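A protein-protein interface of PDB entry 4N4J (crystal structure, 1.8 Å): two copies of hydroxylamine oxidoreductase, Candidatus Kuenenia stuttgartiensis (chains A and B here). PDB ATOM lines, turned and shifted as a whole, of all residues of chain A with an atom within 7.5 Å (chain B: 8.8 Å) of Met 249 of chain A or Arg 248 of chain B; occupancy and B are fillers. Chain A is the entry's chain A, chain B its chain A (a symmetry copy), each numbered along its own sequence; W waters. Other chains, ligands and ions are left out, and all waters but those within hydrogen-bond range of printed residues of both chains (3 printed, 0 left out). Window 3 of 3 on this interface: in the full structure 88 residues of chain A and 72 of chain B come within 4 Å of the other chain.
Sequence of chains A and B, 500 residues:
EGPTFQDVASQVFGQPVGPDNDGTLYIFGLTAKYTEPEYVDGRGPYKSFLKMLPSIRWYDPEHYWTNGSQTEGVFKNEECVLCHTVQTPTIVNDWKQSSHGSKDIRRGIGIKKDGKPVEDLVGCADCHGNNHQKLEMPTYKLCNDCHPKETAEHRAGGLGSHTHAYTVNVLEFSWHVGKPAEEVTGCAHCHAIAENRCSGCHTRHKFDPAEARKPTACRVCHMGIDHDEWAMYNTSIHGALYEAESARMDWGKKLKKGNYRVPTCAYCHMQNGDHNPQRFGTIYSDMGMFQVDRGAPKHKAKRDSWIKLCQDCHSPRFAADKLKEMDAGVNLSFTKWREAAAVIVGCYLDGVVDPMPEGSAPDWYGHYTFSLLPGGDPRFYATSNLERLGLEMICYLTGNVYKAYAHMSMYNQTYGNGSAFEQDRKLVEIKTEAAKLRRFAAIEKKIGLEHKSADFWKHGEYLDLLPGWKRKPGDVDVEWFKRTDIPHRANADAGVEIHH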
ATOM      1  N   ARG A 213      16.705  -7.970  17.961  1.00  0.00           N
ATOM      2  CA  ARG A 213      17.591  -8.369  19.057  1.00  0.00           C
ATOM      3  C   ARG A 213      18.711  -7.355  19.322  1.00  0.00           C
ATOM      4  O   ARG A 213      19.299  -7.355  20.393  1.00  0.00           O
ATOM      5  CB  ARG A 213      18.199  -9.741  18.767  1.00  0.00           C
ATOM      6  CG  ARG A 213      17.169 -10.845  18.783  1.00  0.00           C
ATOM      7  CD  ARG A 213      17.728 -12.186  18.374  1.00  0.00           C
ATOM      8  NE  ARG A 213      16.610 -13.100  18.184  1.00  0.00           N
ATOM      9  CZ  ARG A 213      16.318 -13.774  17.076  1.00  0.00           C
ATOM     10  NH1 ARG A 213      17.090 -13.728  15.998  1.00  0.00           N
ATOM     11  NH2 ARG A 213      15.232 -14.537  17.066  1.00  0.00           N
ATOM     12  N   LYS A 214      18.997  -6.501  18.344  1.00  0.00           N
ATOM     13  CA  LYS A 214      20.107  -5.553  18.442  1.00  0.00           C
ATOM     14  C   LYS A 214      19.688  -4.330  19.259  1.00  0.00           C
ATOM     15  O   LYS A 214      18.514  -3.988  19.293  1.00  0.00           O
ATOM     16  CB  LYS A 214      20.557  -5.122  17.042  1.00  0.00           C
ATOM     17  CG  LYS A 214      20.974  -6.295  16.166  1.00  0.00           C
ATOM     18  CD  LYS A 214      21.484  -5.875  14.803  1.00  0.00           C
ATOM     19  CE  LYS A 214      21.767  -7.112  13.949  1.00  0.00           C
ATOM     20  NZ  LYS A 214      22.472  -6.816  12.668  1.00  0.00           N
ATOM     21  N   PRO A 215      20.651  -3.655  19.912  1.00  0.00           N
ATOM     22  CA  PRO A 215      20.334  -2.458  20.694  1.00  0.00           C
ATOM     23  C   PRO A 215      19.744  -1.330  19.855  1.00  0.00           C
ATOM     24  O   PRO A 215      19.052  -0.466  20.378  1.00  0.00           O
ATOM     25  CB  PRO A 215      21.694  -2.036  21.273  1.00  0.00           C
ATOM     26  CG  PRO A 215      22.548  -3.235  21.187  1.00  0.00           C
ATOM     27  CD  PRO A 215      22.076  -4.016  20.011  1.00  0.00           C
ATOM     28  N   LEU A 241      31.425  -4.564  24.203  1.00  0.00           N
ATOM     29  CA  LEU A 241      31.510  -5.879  23.570  1.00  0.00           C
ATOM     30  C   LEU A 241      30.479  -6.034  22.453  1.00  0.00           C
ATOM     31  O   LEU A 241      30.764  -6.652  21.433  1.00  0.00           O
ATOM     32  CB  LEU A 241      31.375  -7.000  24.606  1.00  0.00           C
ATOM     33  CG  LEU A 241      32.553  -7.141  25.571  1.00  0.00           C
ATOM     34  CD1 LEU A 241      32.311  -8.275  26.554  1.00  0.00           C
ATOM     35  CD2 LEU A 241      33.857  -7.370  24.803  1.00  0.00           C
ATOM     36  N   TYR A 242      29.294  -5.453  22.629  1.00  0.00           N
ATOM     37  CA  TYR A 242      28.316  -5.408  21.549  1.00  0.00           C
ATOM     38  C   TYR A 242      28.942  -4.761  20.319  1.00  0.00           C
ATOM     39  O   TYR A 242      28.894  -5.323  19.227  1.00  0.00           O
ATOM     40  CB  TYR A 242      27.043  -4.655  21.962  1.00  0.00           C
ATOM     41  CG  TYR A 242      26.360  -3.983  20.797  1.00  0.00           C
ATOM     42  CD1 TYR A 242      25.746  -4.735  19.805  1.00  0.00           C
ATOM     43  CD2 TYR A 242      26.356  -2.596  20.671  1.00  0.00           C
ATOM     44  CE1 TYR A 242      25.135  -4.127  18.719  1.00  0.00           C
ATOM     45  CE2 TYR A 242      25.739  -1.975  19.592  1.00  0.00           C
ATOM     46  CZ  TYR A 242      25.130  -2.748  18.621  1.00  0.00           C
ATOM     47  OH  TYR A 242      24.518  -2.146  17.546  1.00  0.00           O
ATOM     48  N   GLU A 243      29.543  -3.588  20.494  1.00  0.00           N
ATOM     49  CA  GLU A 243      30.155  -2.893  19.370  1.00  0.00           C
ATOM     50  C   GLU A 243      31.292  -3.723  18.769  1.00  0.00           C
ATOM     51  O   GLU A 243      31.439  -3.794  17.548  1.00  0.00           O
ATOM     52  CB  GLU A 243      30.642  -1.503  19.785  1.00  0.00           C
ATOM     53  CG  GLU A 243      31.384  -0.760  18.690  1.00  0.00           C
ATOM     54  CD  GLU A 243      31.845   0.621  19.101  1.00  0.00           C
ATOM     55  OE1 GLU A 243      31.331   1.167  20.098  1.00  0.00           O
ATOM     56  OE2 GLU A 243      32.729   1.164  18.404  1.00  0.00           O
ATOM     57  N   ALA A 244      32.080  -4.365  19.625  1.00  0.00           N
ATOM     58  CA  ALA A 244      33.192  -5.190  19.156  1.00  0.00           C
ATOM     59  C   ALA A 244      32.720  -6.416  18.368  1.00  0.00           C
ATOM     60  O   ALA A 244      33.343  -6.804  17.378  1.00  0.00           O
ATOM     61  CB  ALA A 244      34.057  -5.620  20.335  1.00  0.00           C
ATOM     62  N   GLU A 245      31.621  -7.025  18.807  1.00  0.00           N
ATOM     63  CA  GLU A 245      31.194  -8.310  18.255  1.00  0.00           C
ATOM     64  C   GLU A 245      30.019  -8.272  17.278  1.00  0.00           C
ATOM     65  O   GLU A 245      29.747  -9.279  16.625  1.00  0.00           O
ATOM     66  CB  GLU A 245      30.877  -9.284  19.398  1.00  0.00           C
ATOM     67  CG  GLU A 245      32.091  -9.545  20.289  1.00  0.00           C
ATOM     68  CD  GLU A 245      31.981 -10.789  21.154  1.00  0.00           C
ATOM     69  OE1 GLU A 245      32.991 -11.119  21.814  1.00  0.00           O
ATOM     70  OE2 GLU A 245      30.915 -11.441  21.174  1.00  0.00           O
ATOM     71  N   SER A 246      29.341  -7.131  17.165  1.00  0.00           N
ATOM     72  CA  SER A 246      28.110  -7.054  16.375  1.00  0.00           C
ATOM     73  C   SER A 246      28.287  -7.499  14.926  1.00  0.00           C
ATOM     74  O   SER A 246      27.415  -8.167  14.369  1.00  0.00           O
ATOM     75  CB  SER A 246      27.533  -5.642  16.394  1.00  0.00           C
ATOM     76  OG  SER A 246      26.384  -5.578  15.570  1.00  0.00           O
ATOM     77  N   ALA A 247      29.413  -7.129  14.322  1.00  0.00           N
ATOM     78  CA  ALA A 247      29.648  -7.393  12.904  1.00  0.00           C
ATOM     79  C   ALA A 247      29.763  -8.875  12.559  1.00  0.00           C
ATOM     80  O   ALA A 247      29.433  -9.277  11.434  1.00  0.00           O
ATOM     81  CB  ALA A 247      30.896  -6.646  12.424  1.00  0.00           C
ATOM     82  N   ARG A 248      30.229  -9.678  13.508  1.00  0.00           N
ATOM     83  CA  ARG A 248      30.547 -11.077  13.231  1.00  0.00           C
ATOM     84  C   ARG A 248      29.744 -12.087  14.050  1.00  0.00           C
ATOM     85  O   ARG A 248      29.797 -13.284  13.771  1.00  0.00           O
ATOM     86  CB  ARG A 248      32.048 -11.295  13.413  1.00  0.00           C
ATOM     87  CG  ARG A 248      32.887 -10.493  12.407  1.00  0.00           C
ATOM     88  CD  ARG A 248      34.342 -10.414  12.817  1.00  0.00           C
ATOM     89  NE  ARG A 248      35.140  -9.571  11.920  1.00  0.00           N
ATOM     90  CZ  ARG A 248      35.246  -8.239  12.000  1.00  0.00           C
ATOM     91  NH1 ARG A 248      34.590  -7.548  12.930  1.00  0.00           N
ATOM     92  NH2 ARG A 248      36.019  -7.588  11.134  1.00  0.00           N
ATOM     93  N   MET A 249      28.995 -11.620  15.042  1.00  0.00           N
ATOM     94  CA  MET A 249      28.221 -12.529  15.884  1.00  0.00           C
ATOM     95  C   MET A 249      26.966 -13.010  15.168  1.00  0.00           C
ATOM     96  O   MET A 249      26.515 -12.414  14.182  1.00  0.00           O
ATOM     97  CB  MET A 249      27.864 -11.880  17.224  1.00  0.00           C
ATOM     98  CG  MET A 249      26.989 -10.651  17.122  1.00  0.00           C
ATOM     99  SD  MET A 249      26.892  -9.808  18.699  1.00  0.00           S
ATOM    100  CE  MET A 249      25.461 -10.654  19.396  1.00  0.00           C
ATOM    101  N   ASP A 250      26.416 -14.107  15.673  1.00  0.00           N
ATOM    102  CA  ASP A 250      25.225 -14.707  15.105  1.00  0.00           C
ATOM    103  C   ASP A 250      23.988 -14.103  15.764  1.00  0.00           C
ATOM    104  O   ASP A 250      23.637 -14.457  16.890  1.00  0.00           O
ATOM    105  CB  ASP A 250      25.258 -16.221  15.312  1.00  0.00           C
ATOM    106  CG  ASP A 250      24.131 -16.939  14.595  1.00  0.00           C
ATOM    107  OD1 ASP A 250      24.129 -18.186  14.629  1.00  0.00           O
ATOM    108  OD2 ASP A 250      23.255 -16.276  13.999  1.00  0.00           O
ATOM    109  N   TRP A 251      23.335 -13.196  15.048  1.00  0.00           N
ATOM    110  CA  TRP A 251      22.127 -12.531  15.539  1.00  0.00           C
ATOM    111  C   TRP A 251      20.865 -13.344  15.257  1.00  0.00           C
ATOM    112  O   TRP A 251      19.770 -12.947  15.641  1.00  0.00           O
ATOM    113  CB  TRP A 251      21.984 -11.158  14.890  1.00  0.00           C
ATOM    114  CG  TRP A 251      22.976 -10.155  15.369  1.00  0.00           C
ATOM    115  CD1 TRP A 251      24.078  -9.706  14.702  1.00  0.00           C
ATOM    116  CD2 TRP A 251      22.945  -9.457  16.615  1.00  0.00           C
ATOM    117  NE1 TRP A 251      24.739  -8.765  15.460  1.00  0.00           N
ATOM    118  CE2 TRP A 251      24.065  -8.598  16.642  1.00  0.00           C
ATOM    119  CE3 TRP A 251      22.079  -9.474  17.718  1.00  0.00           C
ATOM    120  CZ2 TRP A 251      24.342  -7.765  17.726  1.00  0.00           C
ATOM    121  CZ3 TRP A 251      22.358  -8.650  18.794  1.00  0.00           C
ATOM    122  CH2 TRP A 251      23.483  -7.805  18.790  1.00  0.00           C
ATOM    123  N   GLY A 252      21.025 -14.475  14.572  1.00  0.00           N
ATOM    124  CA  GLY A 252      19.901 -15.328  14.206  1.00  0.00           C
ATOM    125  C   GLY A 252      19.449 -16.252  15.320  1.00  0.00           C
ATOM    126  O   GLY A 252      18.450 -16.952  15.168  1.00  0.00           O
ATOM    127  N   ASN A 259      22.982 -18.720  24.109  1.00  0.00           N
ATOM    128  CA  ASN A 259      22.984 -18.352  22.688  1.00  0.00           C
ATOM    129  C   ASN A 259      23.798 -17.103  22.381  1.00  0.00           C
ATOM    130  O   ASN A 259      24.141 -16.865  21.221  1.00  0.00           O
ATOM    131  CB  ASN A 259      21.553 -18.154  22.172  1.00  0.00           C
ATOM    132  CG  ASN A 259      20.851 -19.465  21.873  1.00  0.00           C
ATOM    133  OD1 ASN A 259      21.432 -20.539  22.026  1.00  0.00           O
ATOM    134  ND2 ASN A 259      19.596 -19.381  21.450  1.00  0.00           N
ATOM    135  N   TYR A 260      24.081 -16.307  23.409  1.00  0.00           N
ATOM    136  CA  TYR A 260      24.810 -15.047  23.247  1.00  0.00           C
ATOM    137  C   TYR A 260      25.921 -14.892  24.261  1.00  0.00           C
ATOM    138  O   TYR A 260      25.758 -15.239  25.423  1.00  0.00           O
ATOM    139  CB  TYR A 260      23.843 -13.871  23.380  1.00  0.00           C
ATOM    140  CG  TYR A 260      22.994 -13.741  22.155  1.00  0.00           C
ATOM    141  CD1 TYR A 260      23.415 -12.971  21.083  1.00  0.00           C
ATOM    142  CD2 TYR A 260      21.803 -14.439  22.039  1.00  0.00           C
ATOM    143  CE1 TYR A 260      22.660 -12.875  19.937  1.00  0.00           C
ATOM    144  CE2 TYR A 260      21.038 -14.352  20.898  1.00  0.00           C
ATOM    145  CZ  TYR A 260      21.473 -13.569  19.847  1.00  0.00           C
ATOM    146  OH  TYR A 260      20.725 -13.483  18.700  1.00  0.00           O
ATOM    147  N   ARG A 261      27.047 -14.347  23.815  1.00  0.00           N
ATOM    148  CA  ARG A 261      28.089 -13.930  24.740  1.00  0.00           C
ATOM    149  C   ARG A 261      27.742 -12.558  25.302  1.00  0.00           C
ATOM    150  O   ARG A 261      27.927 -12.302  26.487  1.00  0.00           O
ATOM    151  CB  ARG A 261      29.447 -13.846  24.052  1.00  0.00           C
ATOM    152  CG  ARG A 261      30.533 -13.437  25.025  1.00  0.00           C
ATOM    153  CD  ARG A 261      31.868 -13.194  24.374  1.00  0.00           C
ATOM    154  NE  ARG A 261      32.877 -13.016  25.415  1.00  0.00           N
ATOM    155  CZ  ARG A 261      33.878 -12.143  25.386  1.00  0.00           C
ATOM    156  NH1 ARG A 261      34.048 -11.299  24.366  1.00  0.00           N
ATOM    157  NH2 ARG A 261      34.712 -12.101  26.418  1.00  0.00           N
ATOM    158  N   VAL A 262      27.277 -11.671  24.430  1.00  0.00           N
ATOM    159  CA  VAL A 262      27.023 -10.291  24.800  1.00  0.00           C
ATOM    160  C   VAL A 262      25.524 -10.073  24.941  1.00  0.00           C
ATOM    161  O   VAL A 262      24.774 -10.353  24.006  1.00  0.00           O
ATOM    162  CB  VAL A 262      27.582  -9.328  23.741  1.00  0.00           C
ATOM    163  CG1 VAL A 262      27.234  -7.883  24.100  1.00  0.00           C
ATOM    164  CG2 VAL A 262      29.095  -9.494  23.628  1.00  0.00           C
ATOM    165  N   PRO A 263      25.082  -9.563  26.104  1.00  0.00           N
ATOM    166  CA  PRO A 263      23.670  -9.295  26.284  1.00  0.00           C
ATOM    167  C   PRO A 263      23.289  -7.950  25.683  1.00  0.00           C
ATOM    168  O   PRO A 263      24.035  -6.984  25.802  1.00  0.00           O
ATOM    169  CB  PRO A 263      23.521  -9.255  27.802  1.00  0.00           C
ATOM    170  CG  PRO A 263      24.814  -8.706  28.270  1.00  0.00           C
ATOM    171  CD  PRO A 263      25.857  -9.191  27.301  1.00  0.00           C
ATOM    172  N   THR A 264      22.130  -7.907  25.044  1.00  0.00           N
ATOM    173  CA  THR A 264      21.559  -6.668  24.535  1.00  0.00           C
ATOM    174  C   THR A 264      20.317  -6.333  25.342  1.00  0.00           C
ATOM    175  O   THR A 264      19.889  -7.124  26.194  1.00  0.00           O
ATOM    176  CB  THR A 264      21.134  -6.826  23.072  1.00  0.00           C
ATOM    177  OG1 THR A 264      20.120  -7.839  22.984  1.00  0.00           O
ATOM    178  CG2 THR A 264      22.324  -7.210  22.198  1.00  0.00           C
ATOM    179  N   LYS B 214      29.030   5.807   3.204  1.00  0.00           N
ATOM    180  CA  LYS B 214      28.723   5.588   4.618  1.00  0.00           C
ATOM    181  C   LYS B 214      28.620   6.926   5.352  1.00  0.00           C
ATOM    182  O   LYS B 214      29.246   7.896   4.948  1.00  0.00           O
ATOM    183  CB  LYS B 214      29.804   4.715   5.263  1.00  0.00           C
ATOM    184  CG  LYS B 214      29.973   3.370   4.570  1.00  0.00           C
ATOM    185  CD  LYS B 214      30.993   2.473   5.240  1.00  0.00           C
ATOM    186  CE  LYS B 214      31.186   1.198   4.417  1.00  0.00           C
ATOM    187  NZ  LYS B 214      32.008   0.156   5.097  1.00  0.00           N
ATOM    188  N   LEU B 241      18.964   1.749  11.851  1.00  0.00           N
ATOM    189  CA  LEU B 241      19.042   0.691  10.844  1.00  0.00           C
ATOM    190  C   LEU B 241      20.402   0.678  10.145  1.00  0.00           C
ATOM    191  O   LEU B 241      20.922  -0.387   9.832  1.00  0.00           O
ATOM    192  CB  LEU B 241      17.901   0.811   9.828  1.00  0.00           C
ATOM    193  CG  LEU B 241      16.508   0.496  10.374  1.00  0.00           C
ATOM    194  CD1 LEU B 241      15.457   0.651   9.286  1.00  0.00           C
ATOM    195  CD2 LEU B 241      16.463  -0.917  10.961  1.00  0.00           C
ATOM    196  N   TYR B 242      20.990   1.852   9.928  1.00  0.00           N
ATOM    197  CA  TYR B 242      22.356   1.922   9.423  1.00  0.00           C
ATOM    198  C   TYR B 242      23.281   1.133  10.341  1.00  0.00           C
ATOM    199  O   TYR B 242      24.034   0.278   9.881  1.00  0.00           O
ATOM    200  CB  TYR B 242      22.842   3.372   9.288  1.00  0.00           C
ATOM    201  CG  TYR B 242      24.333   3.506   9.467  1.00  0.00           C
ATOM    202  CD1 TYR B 242      25.210   2.991   8.521  1.00  0.00           C
ATOM    203  CD2 TYR B 242      24.868   4.119  10.598  1.00  0.00           C
ATOM    204  CE1 TYR B 242      26.582   3.089   8.688  1.00  0.00           C
ATOM    205  CE2 TYR B 242      26.242   4.232  10.771  1.00  0.00           C
ATOM    206  CZ  TYR B 242      27.092   3.715   9.810  1.00  0.00           C
ATOM    207  OH  TYR B 242      28.455   3.817   9.972  1.00  0.00           O
ATOM    208  N   GLU B 243      23.218   1.407  11.641  1.00  0.00           N
ATOM    209  CA  GLU B 243      24.077   0.710  12.589  1.00  0.00           C
ATOM    210  C   GLU B 243      23.787  -0.792  12.586  1.00  0.00           C
ATOM    211  O   GLU B 243      24.708  -1.609  12.642  1.00  0.00           O
ATOM    212  CB  GLU B 243      23.935   1.300  13.993  1.00  0.00           C
ATOM    213  CG  GLU B 243      24.725   0.558  15.055  1.00  0.00           C
ATOM    214  CD  GLU B 243      24.596   1.158  16.436  1.00  0.00           C
ATOM    215  OE1 GLU B 243      24.179   2.328  16.560  1.00  0.00           O
ATOM    216  OE2 GLU B 243      24.927   0.445  17.408  1.00  0.00           O
ATOM    217  N   ALA B 244      22.511  -1.154  12.500  1.00  0.00           N
ATOM    218  CA  ALA B 244      22.124  -2.564  12.484  1.00  0.00           C
ATOM    219  C   ALA B 244      22.619  -3.292  11.230  1.00  0.00           C
ATOM    220  O   ALA B 244      23.027  -4.453  11.299  1.00  0.00           O
ATOM    221  CB  ALA B 244      20.610  -2.692  12.608  1.00  0.00           C
ATOM    222  N   GLU B 245      22.581  -2.612  10.087  1.00  0.00           N
ATOM    223  CA  GLU B 245      22.841  -3.268   8.806  1.00  0.00           C
ATOM    224  C   GLU B 245      24.211  -3.013   8.179  1.00  0.00           C
ATOM    225  O   GLU B 245      24.568  -3.692   7.216  1.00  0.00           O
ATOM    226  CB  GLU B 245      21.741  -2.895   7.803  1.00  0.00           C
ATOM    227  CG  GLU B 245      20.356  -3.334   8.272  1.00  0.00           C
ATOM    228  CD  GLU B 245      19.306  -3.388   7.175  1.00  0.00           C
ATOM    229  OE1 GLU B 245      18.185  -3.854   7.476  1.00  0.00           O
ATOM    230  OE2 GLU B 245      19.586  -2.985   6.026  1.00  0.00           O
ATOM    231  N   SER B 246      24.974  -2.063   8.718  1.00  0.00           N
ATOM    232  CA  SER B 246      26.228  -1.647   8.085  1.00  0.00           C
ATOM    233  C   SER B 246      27.208  -2.795   7.860  1.00  0.00           C
ATOM    234  O   SER B 246      27.870  -2.853   6.822  1.00  0.00           O
ATOM    235  CB  SER B 246      26.918  -0.557   8.899  1.00  0.00           C
ATOM    236  OG  SER B 246      28.158  -0.221   8.305  1.00  0.00           O
ATOM    237  N   ALA B 247      27.296  -3.703   8.828  1.00  0.00           N
ATOM    238  CA  ALA B 247      28.279  -4.783   8.782  1.00  0.00           C
ATOM    239  C   ALA B 247      28.053  -5.781   7.650  1.00  0.00           C
ATOM    240  O   ALA B 247      29.014  -6.388   7.158  1.00  0.00           O
ATOM    241  CB  ALA B 247      28.323  -5.517  10.125  1.00  0.00           C
ATOM    242  N   ARG B 248      26.800  -5.955   7.244  1.00  0.00           N
ATOM    243  CA  ARG B 248      26.449  -7.009   6.296  1.00  0.00           C
ATOM    244  C   ARG B 248      25.834  -6.511   4.988  1.00  0.00           C
ATOM    245  O   ARG B 248      25.671  -7.291   4.051  1.00  0.00           O
ATOM    246  CB  ARG B 248      25.529  -8.016   6.984  1.00  0.00           C
ATOM    247  CG  ARG B 248      26.218  -8.745   8.148  1.00  0.00           C
ATOM    248  CD  ARG B 248      25.222  -9.447   9.046  1.00  0.00           C
ATOM    249  NE  ARG B 248      25.852 -10.067  10.217  1.00  0.00           N
ATOM    250  CZ  ARG B 248      26.148  -9.440  11.360  1.00  0.00           C
ATOM    251  NH1 ARG B 248      25.898  -8.142  11.521  1.00  0.00           N
ATOM    252  NH2 ARG B 248      26.705 -10.121  12.360  1.00  0.00           N
ATOM    253  N   MET B 249      25.507  -5.227   4.911  1.00  0.00           N
ATOM    254  CA  MET B 249      24.891  -4.685   3.702  1.00  0.00           C
ATOM    255  C   MET B 249      25.923  -4.485   2.599  1.00  0.00           C
ATOM    256  O   MET B 249      27.134  -4.444   2.846  1.00  0.00           O
ATOM    257  CB  MET B 249      24.149  -3.378   3.992  1.00  0.00           C
ATOM    258  CG  MET B 249      25.022  -2.248   4.488  1.00  0.00           C
ATOM    259  SD  MET B 249      24.023  -0.885   5.081  1.00  0.00           S
ATOM    260  CE  MET B 249      23.853   0.044   3.546  1.00  0.00           C
ATOM    261  N   ASP B 250      25.423  -4.374   1.376  1.00  0.00           N
ATOM    262  CA  ASP B 250      26.265  -4.193   0.209  1.00  0.00           C
ATOM    263  C   ASP B 250      26.484  -2.702  -0.032  1.00  0.00           C
ATOM    264  O   ASP B 250      25.606  -2.010  -0.550  1.00  0.00           O
ATOM    265  CB  ASP B 250      25.609  -4.842  -1.009  1.00  0.00           C
ATOM    266  CG  ASP B 250      26.509  -4.844  -2.231  1.00  0.00           C
ATOM    267  OD1 ASP B 250      26.097  -5.437  -3.248  1.00  0.00           O
ATOM    268  OD2 ASP B 250      27.617  -4.268  -2.185  1.00  0.00           O
ATOM    269  N   TRP B 251      27.662  -2.221   0.346  1.00  0.00           N
ATOM    270  CA  TRP B 251      28.026  -0.814   0.175  1.00  0.00           C
ATOM    271  C   TRP B 251      28.599  -0.530  -1.212  1.00  0.00           C
ATOM    272  O   TRP B 251      28.915   0.612  -1.532  1.00  0.00           O
ATOM    273  CB  TRP B 251      29.055  -0.407   1.226  1.00  0.00           C
ATOM    274  CG  TRP B 251      28.504  -0.308   2.606  1.00  0.00           C
ATOM    275  CD1 TRP B 251      28.680  -1.196   3.627  1.00  0.00           C
ATOM    276  CD2 TRP B 251      27.702   0.753   3.128  1.00  0.00           C
ATOM    277  NE1 TRP B 251      28.034  -0.750   4.758  1.00  0.00           N
ATOM    278  CE2 TRP B 251      27.422   0.443   4.476  1.00  0.00           C
ATOM    279  CE3 TRP B 251      27.189   1.940   2.585  1.00  0.00           C
ATOM    280  CZ2 TRP B 251      26.652   1.275   5.289  1.00  0.00           C
ATOM    281  CZ3 TRP B 251      26.422   2.762   3.393  1.00  0.00           C
ATOM    282  CH2 TRP B 251      26.159   2.424   4.734  1.00  0.00           C
HETATM  283  O   HOH W   1      20.102  -6.191  11.026  1.00  0.00           O
HETATM  284  O   HOH W   2      25.155  -6.014  13.184  1.00  0.00           O
HETATM  285  O   HOH W   3      25.076  -3.450  15.088  1.00  0.00           O
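Lys 214 of chain A touches Ala 244 of chain B, but with the chains exchanged Ala 244 of chain A does not touch Lys 214 of chain B (14.2 Å). Tyr 242 of chain A touches Glu 243 of chain B, but with the chains exchanged Glu 243 of chain A does not touch Tyr 242 of chain B (9.8 Å). Ala 247 of chain A touches Arg 248 of chain B, but with the chains exchanged Arg 248 of chain A does not touch Ala 247 of chain B (5.7 Å). Arg 248 of chain A touches its own counterpart, Arg 248 of chain B. 12 positions are printed for both chains. Of the 9 pairs that touch across the chains among the printed residues, 2 have their exchanged pair printed and touching as well.
The backbone carbonyl oxygen (O) of Met 249 of chain A is in hydrogen-bond range of the guanidinium group (NH2) of Arg 248 of chain B (2.9 Å). The backbone carbonyl oxygen of Ser 246 of chain A sits at hydrogen-bond distance from the guanidinium group of Arg 248 of chain B (2.9 Å). The side-chain hydroxyl of Tyr 242 of chain A sits at hydrogen-bond distance from the side-chain carboxylate of Glu 243 of chain B (2.6 Å). The backbone carbonyl oxygen (O) of Ala 244 of chain B lies within hydrogen-bond range of the side-chain amino group (NZ) of Lys 214 of chain A (2.8 Å). O of Ala 247 of chain A lies within hydrogen-bond range of NH2 of Arg 248 of chain B (3.0 Å).
Water W3 lies within hydrogen-bond range of OG of Ser 246 of chain A (2.5 Å), OH of Tyr 242 of chain A (2.8 Å) and O of Glu 243 of chain B (3.1 Å). Water W2 lies within hydrogen-bond range of OG of Ser 246 of chain A (2.7 Å), NH1 of Arg 248 of chain B (2.8 Å), NZ of Lys 214 of chain A (2.8 Å) and O of Ala 244 of chain B (3.2 Å). Water W1 lies within hydrogen-bond range of NZ of Lys 214 of chain A and O of Ala 244 of chain B.
Arg 248 of chain B touches Lys 214 of chain A (NH1 to NZ, 3.8 Å). CB of Ala 247 of chain B touches CA of Ala 247 of chain A, 3.6 Å away. N of Arg 248 of chain A touches NH2 of Arg 248 of chain B, at 3.7 Å. CD1 of Trp 251 of chain A touches NH2 of Arg 248 of chain B, at 3.5 Å.
Of chain B, only Arg 248 comes within 4 Å of Met 249 of chain A. Printed residues of chain A within 4 Å of Arg 248 of chain B: Lys 214 (3.8 Å), Ser 246 (2.9 Å), Ala 247 (3.0 Å), Arg 248 (3.7 Å), Met 249 (2.9 Å) and Trp 251 (3.5 Å). Of chain A, only Ala 247 (3.6 Å) comes within 4 Å of Ala 247 of chain B. Of the printed residues of chain B, Trp 251 of chain A touches Arg 248 (3.5 Å). Of the printed residues of chain A, Glu 243 of chain B touches Tyr 242 (2.6 Å). Leu 241 of chain A touches none of the printed residues of chain B. Val 262 of chain A touches none of the printed residues of chain B. The nearest printed residue of chain B that does not touch Tyr 242 of chain A is Ala 244 of chain B (5.5 Å).
Printed residues of chain B that touch a printed residue of chain A: Glu 243, Ala 244, Ala 247 and Arg 248. Of the 21 printed residues of chain A, 7 touch a printed residue of chain B. Hydrophobic or aromatic side chains of chain A within 4 Å of the printed part of chain B: Tyr 242, Ala 247 and Trp 251. Among the printed residues, no Asp or Glu carboxylate lies within 4 Å of a Lys or Arg side-chain nitrogen of the other chain.
The guanidinium group (NH1) of Arg 213 of chain A lies within hydrogen-bond range of the backbone carbonyl oxygen (O) of Trp 251 of chain A (2.8 Å). O of Trp 251 of chain A sits at hydrogen-bond distance from OH of Tyr 260 of chain A, at 3.2 Å. NE1 of Trp 251 of chain A is in hydrogen-bond range of O of Ser 246 of chain A (3.0 Å).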
